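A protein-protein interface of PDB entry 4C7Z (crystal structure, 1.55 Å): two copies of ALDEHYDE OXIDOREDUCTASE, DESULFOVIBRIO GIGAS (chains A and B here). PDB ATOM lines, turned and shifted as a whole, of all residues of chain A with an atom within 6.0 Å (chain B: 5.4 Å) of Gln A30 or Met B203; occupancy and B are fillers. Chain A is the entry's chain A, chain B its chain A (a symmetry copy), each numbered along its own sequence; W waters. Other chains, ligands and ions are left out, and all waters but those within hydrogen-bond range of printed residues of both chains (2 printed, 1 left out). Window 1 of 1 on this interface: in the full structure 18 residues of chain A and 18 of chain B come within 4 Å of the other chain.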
ATOM      1  N   MET A   1      -4.887   8.320   0.110  1.00  0.00           N
ATOM      2  CA  MET A   1      -4.794   9.709   0.716  1.00  0.00           C
ATOM      3  C   MET A   1      -4.716   9.497   2.221  1.00  0.00           C
ATOM      4  O   MET A   1      -5.176   8.471   2.749  1.00  0.00           O
ATOM      5  CB  MET A   1      -6.071  10.509   0.368  1.00  0.00           C
ATOM      6  CG  MET A   1      -6.261  11.780   1.204  1.00  0.00           C
ATOM      7  SD  MET A   1      -7.599  12.811   0.558  1.00  0.00           S
ATOM      8  CE  MET A   1      -6.770  13.739  -0.680  1.00  0.00           C
ATOM      9  N   LEU A  15      -4.392  18.610   7.267  1.00  0.00           N
ATOM     10  CA  LEU A  15      -3.973  18.389   5.891  1.00  0.00           C
ATOM     11  C   LEU A  15      -4.466  17.093   5.337  1.00  0.00           C
ATOM     12  O   LEU A  15      -4.482  16.085   6.034  1.00  0.00           O
ATOM     13  CB  LEU A  15      -2.454  18.342   5.774  1.00  0.00           C
ATOM     14  CG  LEU A  15      -1.695  19.611   6.007  1.00  0.00           C
ATOM     15  CD1 LEU A  15      -0.217  19.290   5.741  1.00  0.00           C
ATOM     16  CD2 LEU A  15      -2.197  20.722   5.099  1.00  0.00           C
ATOM     17  N   PHE A  16      -4.835  17.133   4.070  1.00  0.00           N
ATOM     18  CA  PHE A  16      -5.236  15.921   3.329  1.00  0.00           C
ATOM     19  C   PHE A  16      -4.311  15.828   2.135  1.00  0.00           C
ATOM     20  O   PHE A  16      -4.337  16.681   1.256  1.00  0.00           O
ATOM     21  CB  PHE A  16      -6.700  16.009   2.960  1.00  0.00           C
ATOM     22  CG  PHE A  16      -7.570  15.950   4.181  1.00  0.00           C
ATOM     23  CD1 PHE A  16      -7.839  17.122   4.886  1.00  0.00           C
ATOM     24  CD2 PHE A  16      -7.959  14.741   4.723  1.00  0.00           C
ATOM     25  CE1 PHE A  16      -8.561  17.074   6.039  1.00  0.00           C
ATOM     26  CE2 PHE A  16      -8.707  14.689   5.905  1.00  0.00           C
ATOM     27  CZ  PHE A  16      -8.965  15.871   6.577  1.00  0.00           C
ATOM     28  N   VAL A  17      -3.492  14.783   2.136  1.00  0.00           N
ATOM     29  CA  VAL A  17      -2.419  14.666   1.165  1.00  0.00           C
ATOM     30  C   VAL A  17      -2.248  13.229   0.643  1.00  0.00           C
ATOM     31  O   VAL A  17      -2.665  12.263   1.259  1.00  0.00           O
ATOM     32  CB  VAL A  17      -1.068  15.144   1.749  1.00  0.00           C
ATOM     33  CG1 VAL A  17      -1.116  16.650   2.066  1.00  0.00           C
ATOM     34  CG2 VAL A  17      -0.682  14.320   2.958  1.00  0.00           C
ATOM     35  N   ASP A  18      -1.587  13.148  -0.519  1.00  0.00           N
ATOM     36  CA  ASP A  18      -1.031  11.907  -1.057  1.00  0.00           C
ATOM     37  C   ASP A  18       0.319  11.760  -0.347  1.00  0.00           C
ATOM     38  O   ASP A  18       1.121  12.701  -0.283  1.00  0.00           O
ATOM     39  CB  ASP A  18      -0.840  12.078  -2.565  1.00  0.00           C
ATOM     40  CG  ASP A  18      -0.218  10.842  -3.285  1.00  0.00           C
ATOM     41  OD1 ASP A  18       0.212   9.854  -2.655  1.00  0.00           O
ATOM     42  OD2 ASP A  18      -0.164  10.911  -4.548  1.00  0.00           O
ATOM     43  N   ALA A  21       3.209  12.739  -2.374  1.00  0.00           N
ATOM     44  CA  ALA A  21       3.342  14.091  -2.832  1.00  0.00           C
ATOM     45  C   ALA A  21       4.556  14.760  -2.221  1.00  0.00           C
ATOM     46  O   ALA A  21       4.921  14.483  -1.076  1.00  0.00           O
ATOM     47  CB  ALA A  21       2.084  14.900  -2.522  1.00  0.00           C
ATOM     48  N   ASP A  25       5.124  21.002  -3.288  1.00  0.00           N
ATOM     49  CA  ASP A  25       3.831  21.114  -3.962  1.00  0.00           C
ATOM     50  C   ASP A  25       2.712  21.307  -2.963  1.00  0.00           C
ATOM     51  O   ASP A  25       1.802  22.102  -3.182  1.00  0.00           O
ATOM     52  CB  ASP A  25       3.554  19.886  -4.831  1.00  0.00           C
ATOM     53  CG  ASP A  25       4.432  19.839  -6.080  1.00  0.00           C
ATOM     54  OD1 ASP A  25       4.830  20.898  -6.615  1.00  0.00           O
ATOM     55  OD2 ASP A  25       4.733  18.714  -6.517  1.00  0.00           O
ATOM     56  N   VAL A  26       2.737  20.562  -1.870  1.00  0.00           N
ATOM     57  CA  VAL A  26       1.706  20.708  -0.847  1.00  0.00           C
ATOM     58  C   VAL A  26       1.706  22.130  -0.296  1.00  0.00           C
ATOM     59  O   VAL A  26       0.639  22.777  -0.211  1.00  0.00           O
ATOM     60  CB  VAL A  26       1.872  19.675   0.266  1.00  0.00           C
ATOM     61  CG1 VAL A  26       0.885  19.913   1.436  1.00  0.00           C
ATOM     62  CG2 VAL A  26       1.688  18.268  -0.328  1.00  0.00           C
ATOM     63  N   LEU A  27       2.874  22.603   0.119  1.00  0.00           N
ATOM     64  CA  LEU A  27       2.970  23.945   0.690  1.00  0.00           C
ATOM     65  C   LEU A  27       2.558  25.047  -0.305  1.00  0.00           C
ATOM     66  O   LEU A  27       1.730  25.899   0.026  1.00  0.00           O
ATOM     67  CB  LEU A  27       4.387  24.184   1.220  1.00  0.00           C
ATOM     68  CG  LEU A  27       4.840  23.296   2.390  1.00  0.00           C
ATOM     69  CD1 LEU A  27       6.313  23.551   2.670  1.00  0.00           C
ATOM     70  CD2 LEU A  27       3.983  23.466   3.615  1.00  0.00           C
ATOM     71  N   ARG A  28       3.061  24.963  -1.532  1.00  0.00           N
ATOM     72  CA  ARG A  28       2.784  26.002  -2.546  1.00  0.00           C
ATOM     73  C   ARG A  28       1.340  25.952  -3.060  1.00  0.00           C
ATOM     74  O   ARG A  28       0.666  26.978  -3.132  1.00  0.00           O
ATOM     75  CB  ARG A  28       3.748  25.888  -3.722  1.00  0.00           C
ATOM     76  CG  ARG A  28       5.173  26.283  -3.426  1.00  0.00           C
ATOM     77  CD  ARG A  28       6.112  26.051  -4.593  1.00  0.00           C
ATOM     78  NE  ARG A  28       5.715  26.786  -5.810  1.00  0.00           N
ATOM     79  CZ  ARG A  28       5.866  28.091  -6.007  1.00  0.00           C
ATOM     80  NH1 ARG A  28       6.418  28.878  -5.066  1.00  0.00           N
ATOM     81  NH2 ARG A  28       5.416  28.661  -7.139  1.00  0.00           N
ATOM     82  N   GLN A  29       0.896  24.767  -3.477  1.00  0.00           N
ATOM     83  CA  GLN A  29      -0.371  24.591  -4.183  1.00  0.00           C
ATOM     84  C   GLN A  29      -1.554  24.408  -3.249  1.00  0.00           C
ATOM     85  O   GLN A  29      -2.607  25.055  -3.433  1.00  0.00           O
ATOM     86  CB  GLN A  29      -0.283  23.417  -5.131  1.00  0.00           C
ATOM     87  CG  GLN A  29       0.821  23.647  -6.133  1.00  0.00           C
ATOM     88  CD  GLN A  29       0.898  22.570  -7.188  1.00  0.00           C
ATOM     89  OE1 GLN A  29      -0.120  22.120  -7.683  1.00  0.00           O
ATOM     90  NE2 GLN A  29       2.121  22.169  -7.557  1.00  0.00           N
ATOM     91  N   GLN A  30      -1.438  23.517  -2.260  1.00  0.00           N
ATOM     92  CA  GLN A  30      -2.538  23.272  -1.346  1.00  0.00           C
ATOM     93  C   GLN A  30      -2.671  24.359  -0.287  1.00  0.00           C
ATOM     94  O   GLN A  30      -3.820  24.725   0.080  1.00  0.00           O
ATOM     95  CB  GLN A  30      -2.422  21.888  -0.689  1.00  0.00           C
ATOM     96  CG  GLN A  30      -2.608  20.760  -1.718  1.00  0.00           C
ATOM     97  CD  GLN A  30      -2.465  19.369  -1.134  1.00  0.00           C
ATOM     98  OE1 GLN A  30      -1.564  18.613  -1.538  1.00  0.00           O
ATOM     99  NE2 GLN A  30      -3.265  19.056  -0.145  1.00  0.00           N
ATOM    100  N   LEU A  31      -1.540  24.863   0.220  1.00  0.00           N
ATOM    101  CA  LEU A  31      -1.582  25.888   1.295  1.00  0.00           C
ATOM    102  C   LEU A  31      -1.308  27.311   0.826  1.00  0.00           C
ATOM    103  O   LEU A  31      -1.401  28.216   1.630  1.00  0.00           O
ATOM    104  CB  LEU A  31      -0.646  25.507   2.446  1.00  0.00           C
ATOM    105  CG  LEU A  31      -0.942  24.118   3.063  1.00  0.00           C
ATOM    106  CD1 LEU A  31      -0.020  23.907   4.257  1.00  0.00           C
ATOM    107  CD2 LEU A  31      -2.413  23.966   3.468  1.00  0.00           C
ATOM    108  N   GLY A  32      -0.966  27.506  -0.440  1.00  0.00           N
ATOM    109  CA  GLY A  32      -0.737  28.841  -0.970  1.00  0.00           C
ATOM    110  C   GLY A  32       0.528  29.512  -0.472  1.00  0.00           C
ATOM    111  O   GLY A  32       0.674  30.744  -0.588  1.00  0.00           O
ATOM    112  N   LEU B 199     -11.494  22.995   3.482  1.00  0.00           N
ATOM    113  CA  LEU B 199     -10.680  21.794   3.305  1.00  0.00           C
ATOM    114  C   LEU B 199     -10.688  21.337   1.833  1.00  0.00           C
ATOM    115  O   LEU B 199      -9.651  20.957   1.259  1.00  0.00           O
ATOM    116  CB  LEU B 199     -11.206  20.688   4.239  1.00  0.00           C
ATOM    117  CG  LEU B 199     -10.940  20.943   5.736  1.00  0.00           C
ATOM    118  CD1 LEU B 199     -11.692  19.944   6.609  1.00  0.00           C
ATOM    119  CD2 LEU B 199      -9.437  20.943   6.046  1.00  0.00           C
ATOM    120  N   GLY B 200     -11.841  21.456   1.193  1.00  0.00           N
ATOM    121  CA  GLY B 200     -11.967  21.137  -0.236  1.00  0.00           C
ATOM    122  C   GLY B 200     -11.031  21.954  -1.110  1.00  0.00           C
ATOM    123  O   GLY B 200     -10.449  21.440  -2.082  1.00  0.00           O
ATOM    124  N   LEU B 201     -10.851  23.228  -0.777  1.00  0.00           N
ATOM    125  CA  LEU B 201      -9.936  24.049  -1.555  1.00  0.00           C
ATOM    126  C   LEU B 201      -8.478  23.682  -1.333  1.00  0.00           C
ATOM    127  O   LEU B 201      -7.618  24.035  -2.144  1.00  0.00           O
ATOM    128  CB  LEU B 201     -10.111  25.539  -1.229  1.00  0.00           C
ATOM    129  CG  LEU B 201     -11.439  26.177  -1.667  1.00  0.00           C
ATOM    130  CD1 LEU B 201     -11.428  27.681  -1.408  1.00  0.00           C
ATOM    131  CD2 LEU B 201     -11.775  25.915  -3.121  1.00  0.00           C
ATOM    132  N   LYS B 202      -8.189  23.069  -0.190  1.00  0.00           N
ATOM    133  CA  LYS B 202      -6.828  22.686   0.204  1.00  0.00           C
ATOM    134  C   LYS B 202      -6.508  21.215   0.001  1.00  0.00           C
ATOM    135  O   LYS B 202      -5.485  20.693   0.480  1.00  0.00           O
ATOM    136  CB  LYS B 202      -6.599  23.106   1.659  1.00  0.00           C
ATOM    137  CG  LYS B 202      -6.847  24.594   1.887  1.00  0.00           C
ATOM    138  CD  LYS B 202      -6.685  25.015   3.338  1.00  0.00           C
ATOM    139  CE  LYS B 202      -7.076  26.479   3.463  1.00  0.00           C
ATOM    140  NZ  LYS B 202      -6.723  27.064   4.794  1.00  0.00           N
ATOM    141  N   MET B 203      -7.386  20.538  -0.731  1.00  0.00           N
ATOM    142  CA  MET B 203      -7.166  19.156  -1.093  1.00  0.00           C
ATOM    143  C   MET B 203      -6.299  19.055  -2.356  1.00  0.00           C
ATOM    144  O   MET B 203      -6.155  20.011  -3.120  1.00  0.00           O
ATOM    145  CB  MET B 203      -8.542  18.415  -1.260  1.00  0.00           C
ATOM    146  CG  MET B 203      -9.119  17.915   0.074  1.00  0.00           C
ATOM    147  SD  MET B 203     -10.822  17.325  -0.046  1.00  0.00           S
ATOM    148  CE  MET B 203     -10.485  15.633  -0.528  1.00  0.00           C
ATOM    149  N   PRO B 204      -5.729  17.889  -2.590  1.00  0.00           N
ATOM    150  CA  PRO B 204      -4.810  17.849  -3.734  1.00  0.00           C
ATOM    151  C   PRO B 204      -5.475  17.845  -5.116  1.00  0.00           C
ATOM    152  O   PRO B 204      -6.645  17.530  -5.240  1.00  0.00           O
ATOM    153  CB  PRO B 204      -4.018  16.583  -3.499  1.00  0.00           C
ATOM    154  CG  PRO B 204      -4.767  15.748  -2.564  1.00  0.00           C
ATOM    155  CD  PRO B 204      -5.775  16.639  -1.840  1.00  0.00           C
ATOM    156  N   ALA B 205      -4.638  18.052  -6.137  1.00  0.00           N
ATOM    157  CA  ALA B 205      -5.043  18.121  -7.549  1.00  0.00           C
ATOM    158  C   ALA B 205      -5.925  16.970  -8.008  1.00  0.00           C
ATOM    159  O   ALA B 205      -6.857  17.177  -8.795  1.00  0.00           O
ATOM    160  CB  ALA B 205      -3.799  18.178  -8.429  1.00  0.00           C
ATOM    161  N   THR B 207      -8.214  15.378  -6.597  1.00  0.00           N
ATOM    162  CA  THR B 207      -9.520  15.309  -5.924  1.00  0.00           C
ATOM    163  C   THR B 207     -10.599  15.590  -6.946  1.00  0.00           C
ATOM    164  O   THR B 207     -10.479  16.520  -7.759  1.00  0.00           O
ATOM    165  CB  THR B 207      -9.595  16.323  -4.777  1.00  0.00           C
ATOM    166  OG1 THR B 207      -8.587  16.001  -3.824  1.00  0.00           O
ATOM    167  CG2 THR B 207     -10.938  16.316  -4.080  1.00  0.00           C
ATOM    168  N   PHE B 374     -16.570  15.220   2.396  1.00  0.00           N
ATOM    169  CA  PHE B 374     -15.633  14.596   1.473  1.00  0.00           C
ATOM    170  C   PHE B 374     -15.273  13.199   1.911  1.00  0.00           C
ATOM    171  O   PHE B 374     -15.502  12.833   3.054  1.00  0.00           O
ATOM    172  CB  PHE B 374     -14.395  15.487   1.190  1.00  0.00           C
ATOM    173  CG  PHE B 374     -13.572  15.849   2.400  1.00  0.00           C
ATOM    174  CD1 PHE B 374     -13.833  16.993   3.116  1.00  0.00           C
ATOM    175  CD2 PHE B 374     -12.466  15.078   2.752  1.00  0.00           C
ATOM    176  CE1 PHE B 374     -13.028  17.357   4.207  1.00  0.00           C
ATOM    177  CE2 PHE B 374     -11.685  15.417   3.860  1.00  0.00           C
ATOM    178  CZ  PHE B 374     -11.942  16.574   4.552  1.00  0.00           C
ATOM    179  N   ALA B 375     -14.678  12.426   1.006  1.00  0.00           N
ATOM    180  CA  ALA B 375     -14.291  11.067   1.308  1.00  0.00           C
ATOM    181  C   ALA B 375     -13.099  10.658   0.462  1.00  0.00           C
ATOM    182  O   ALA B 375     -12.829  11.273  -0.568  1.00  0.00           O
ATOM    183  CB  ALA B 375     -15.442  10.109   1.077  1.00  0.00           C
ATOM    184  N   TYR B 376     -12.420   9.598   0.885  1.00  0.00           N
ATOM    185  CA  TYR B 376     -11.260   9.061   0.168  1.00  0.00           C
ATOM    186  C   TYR B 376     -10.961   7.659   0.650  1.00  0.00           C
ATOM    187  O   TYR B 376     -11.411   7.237   1.729  1.00  0.00           O
ATOM    188  CB  TYR B 376     -10.020   9.986   0.360  1.00  0.00           C
ATOM    189  CG  TYR B 376      -9.662  10.207   1.813  1.00  0.00           C
ATOM    190  CD1 TYR B 376      -8.787   9.349   2.481  1.00  0.00           C
ATOM    191  CD2 TYR B 376     -10.197  11.273   2.519  1.00  0.00           C
ATOM    192  CE1 TYR B 376      -8.493   9.551   3.837  1.00  0.00           C
ATOM    193  CE2 TYR B 376      -9.910  11.479   3.861  1.00  0.00           C
ATOM    194  CZ  TYR B 376      -9.072  10.619   4.518  1.00  0.00           C
ATOM    195  OH  TYR B 376      -8.832  10.840   5.869  1.00  0.00           O
ATOM    196  N   PRO B 443     -10.054  10.699  -4.125  1.00  0.00           N
ATOM    197  CA  PRO B 443     -10.722  11.601  -3.205  1.00  0.00           C
ATOM    198  C   PRO B 443     -11.846  12.372  -3.889  1.00  0.00           C
ATOM    199  O   PRO B 443     -11.717  12.754  -5.070  1.00  0.00           O
ATOM    200  CB  PRO B 443      -9.604  12.560  -2.769  1.00  0.00           C
ATOM    201  CG  PRO B 443      -8.312  11.863  -3.129  1.00  0.00           C
ATOM    202  CD  PRO B 443      -8.644  11.068  -4.356  1.00  0.00           C
ATOM    203  N   VAL B 444     -12.947  12.551  -3.180  1.00  0.00           N
ATOM    204  CA  VAL B 444     -14.110  13.266  -3.675  1.00  0.00           C
ATOM    205  C   VAL B 444     -14.571  14.269  -2.653  1.00  0.00           C
ATOM    206  O   VAL B 444     -14.468  14.037  -1.448  1.00  0.00           O
ATOM    207  CB  VAL B 444     -15.256  12.284  -4.037  1.00  0.00           C
ATOM    208  CG1 VAL B 444     -14.814  11.284  -5.086  1.00  0.00           C
ATOM    209  CG2 VAL B 444     -15.788  11.567  -2.816  1.00  0.00           C
ATOM    210  N   HIS B 445     -15.113  15.375  -3.133  1.00  0.00           N
ATOM    211  CA  HIS B 445     -15.613  16.472  -2.298  1.00  0.00           C
ATOM    212  C   HIS B 445     -16.939  16.947  -2.866  1.00  0.00           C
ATOM    213  O   HIS B 445     -17.053  17.164  -4.087  1.00  0.00           O
ATOM    214  CB  HIS B 445     -14.571  17.598  -2.280  1.00  0.00           C
ATOM    215  CG  HIS B 445     -14.875  18.689  -1.312  1.00  0.00           C
ATOM    216  ND1 HIS B 445     -15.762  19.716  -1.584  1.00  0.00           N
ATOM    217  CD2 HIS B 445     -14.424  18.901  -0.057  1.00  0.00           C
ATOM    218  CE1 HIS B 445     -15.823  20.524  -0.541  1.00  0.00           C
ATOM    219  NE2 HIS B 445     -15.065  20.019   0.420  1.00  0.00           N
HETATM  220  O   HOH W   1      -5.414  19.841   3.157  1.00  0.00           O
HETATM  221  O   HOH W   2      -2.119  20.079  -5.673  1.00  0.00           O
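The side-chain amide nitrogen (NE2) of Gln A30 sits at hydrogen-bond distance from the backbone carbonyl oxygen (O) of Lys B202, at 2.8 Å.
NE2 of Gln A30 sits at hydrogen-bond distance from O of Phe A16 (3.0 Å). OG1 of Thr B207 sits at hydrogen-bond distance from O of Pro B204 (2.8 Å).
Among the printed residues, pairs that only touch across the chains: Met A1 with Pro B204, Phe A16 with Pro B204, Met A1 with Pro B443, Met A1 with Tyr B376, Gln A30 with Pro B204, Phe A16 with Phe B374, Gln A30 with Met B203, Phe A16 with Tyr B376 and Phe A16 with Leu B199.
Gln A30 touches just these residues of chain B: Lys B202 (2.8 Å), Met B203 (3.8 Å) and Pro B204 (3.7 Å). Met B203 touches just one residue of chain A: Gln A30. Of the printed residues of chain A, Pro B204 touches Met A1, Phe A16 and Gln A30. Printed residues of chain B within 4 Å of Phe A16: Leu B199 (3.97 Å), Pro B204 (3.4 Å), Phe B374 (3.7 Å) and Tyr B376 (3.9 Å). Printed residues of chain A within 4 Å of Lys B202: Gln A30. Printed residues of chain A within 4 Å of Phe B374: Phe A16 (3.7 Å). Of the printed residues of chain A, Leu B199 touches Phe A16. The nearest residue of chain B that does not touch Gln A30 is Leu B201 (4.5 Å).
Hydrophobic or aromatic side chains of chain B within 4 Å of the printed part of chain A: Leu B199, Pro B204, Phe B374, Tyr B376 and Pro B443. Of the 14 printed residues of chain A, 3 touch a printed residue of chain B. Printed residues of chain A that touch a printed residue of chain B: Met A1, Phe A16 and Gln A30. Along chain A the printed residues that touch a printed residue of chain B span positions 1 to 30. Among the printed residues, no Asp or Glu carboxylate lies within 4 Å of a Lys or Arg side-chain nitrogen of the other chain.
No position is printed for both chains.
Water W1 bridges O of Lys B202 (2.8 Å) and N of Phe A16 (2.9 Å). Water W2 lies within hydrogen-bond range of the backbone NH of Ala B205 (3.3 Å) and the side-chain amide oxygen of Gln A29 (3.5 Å).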
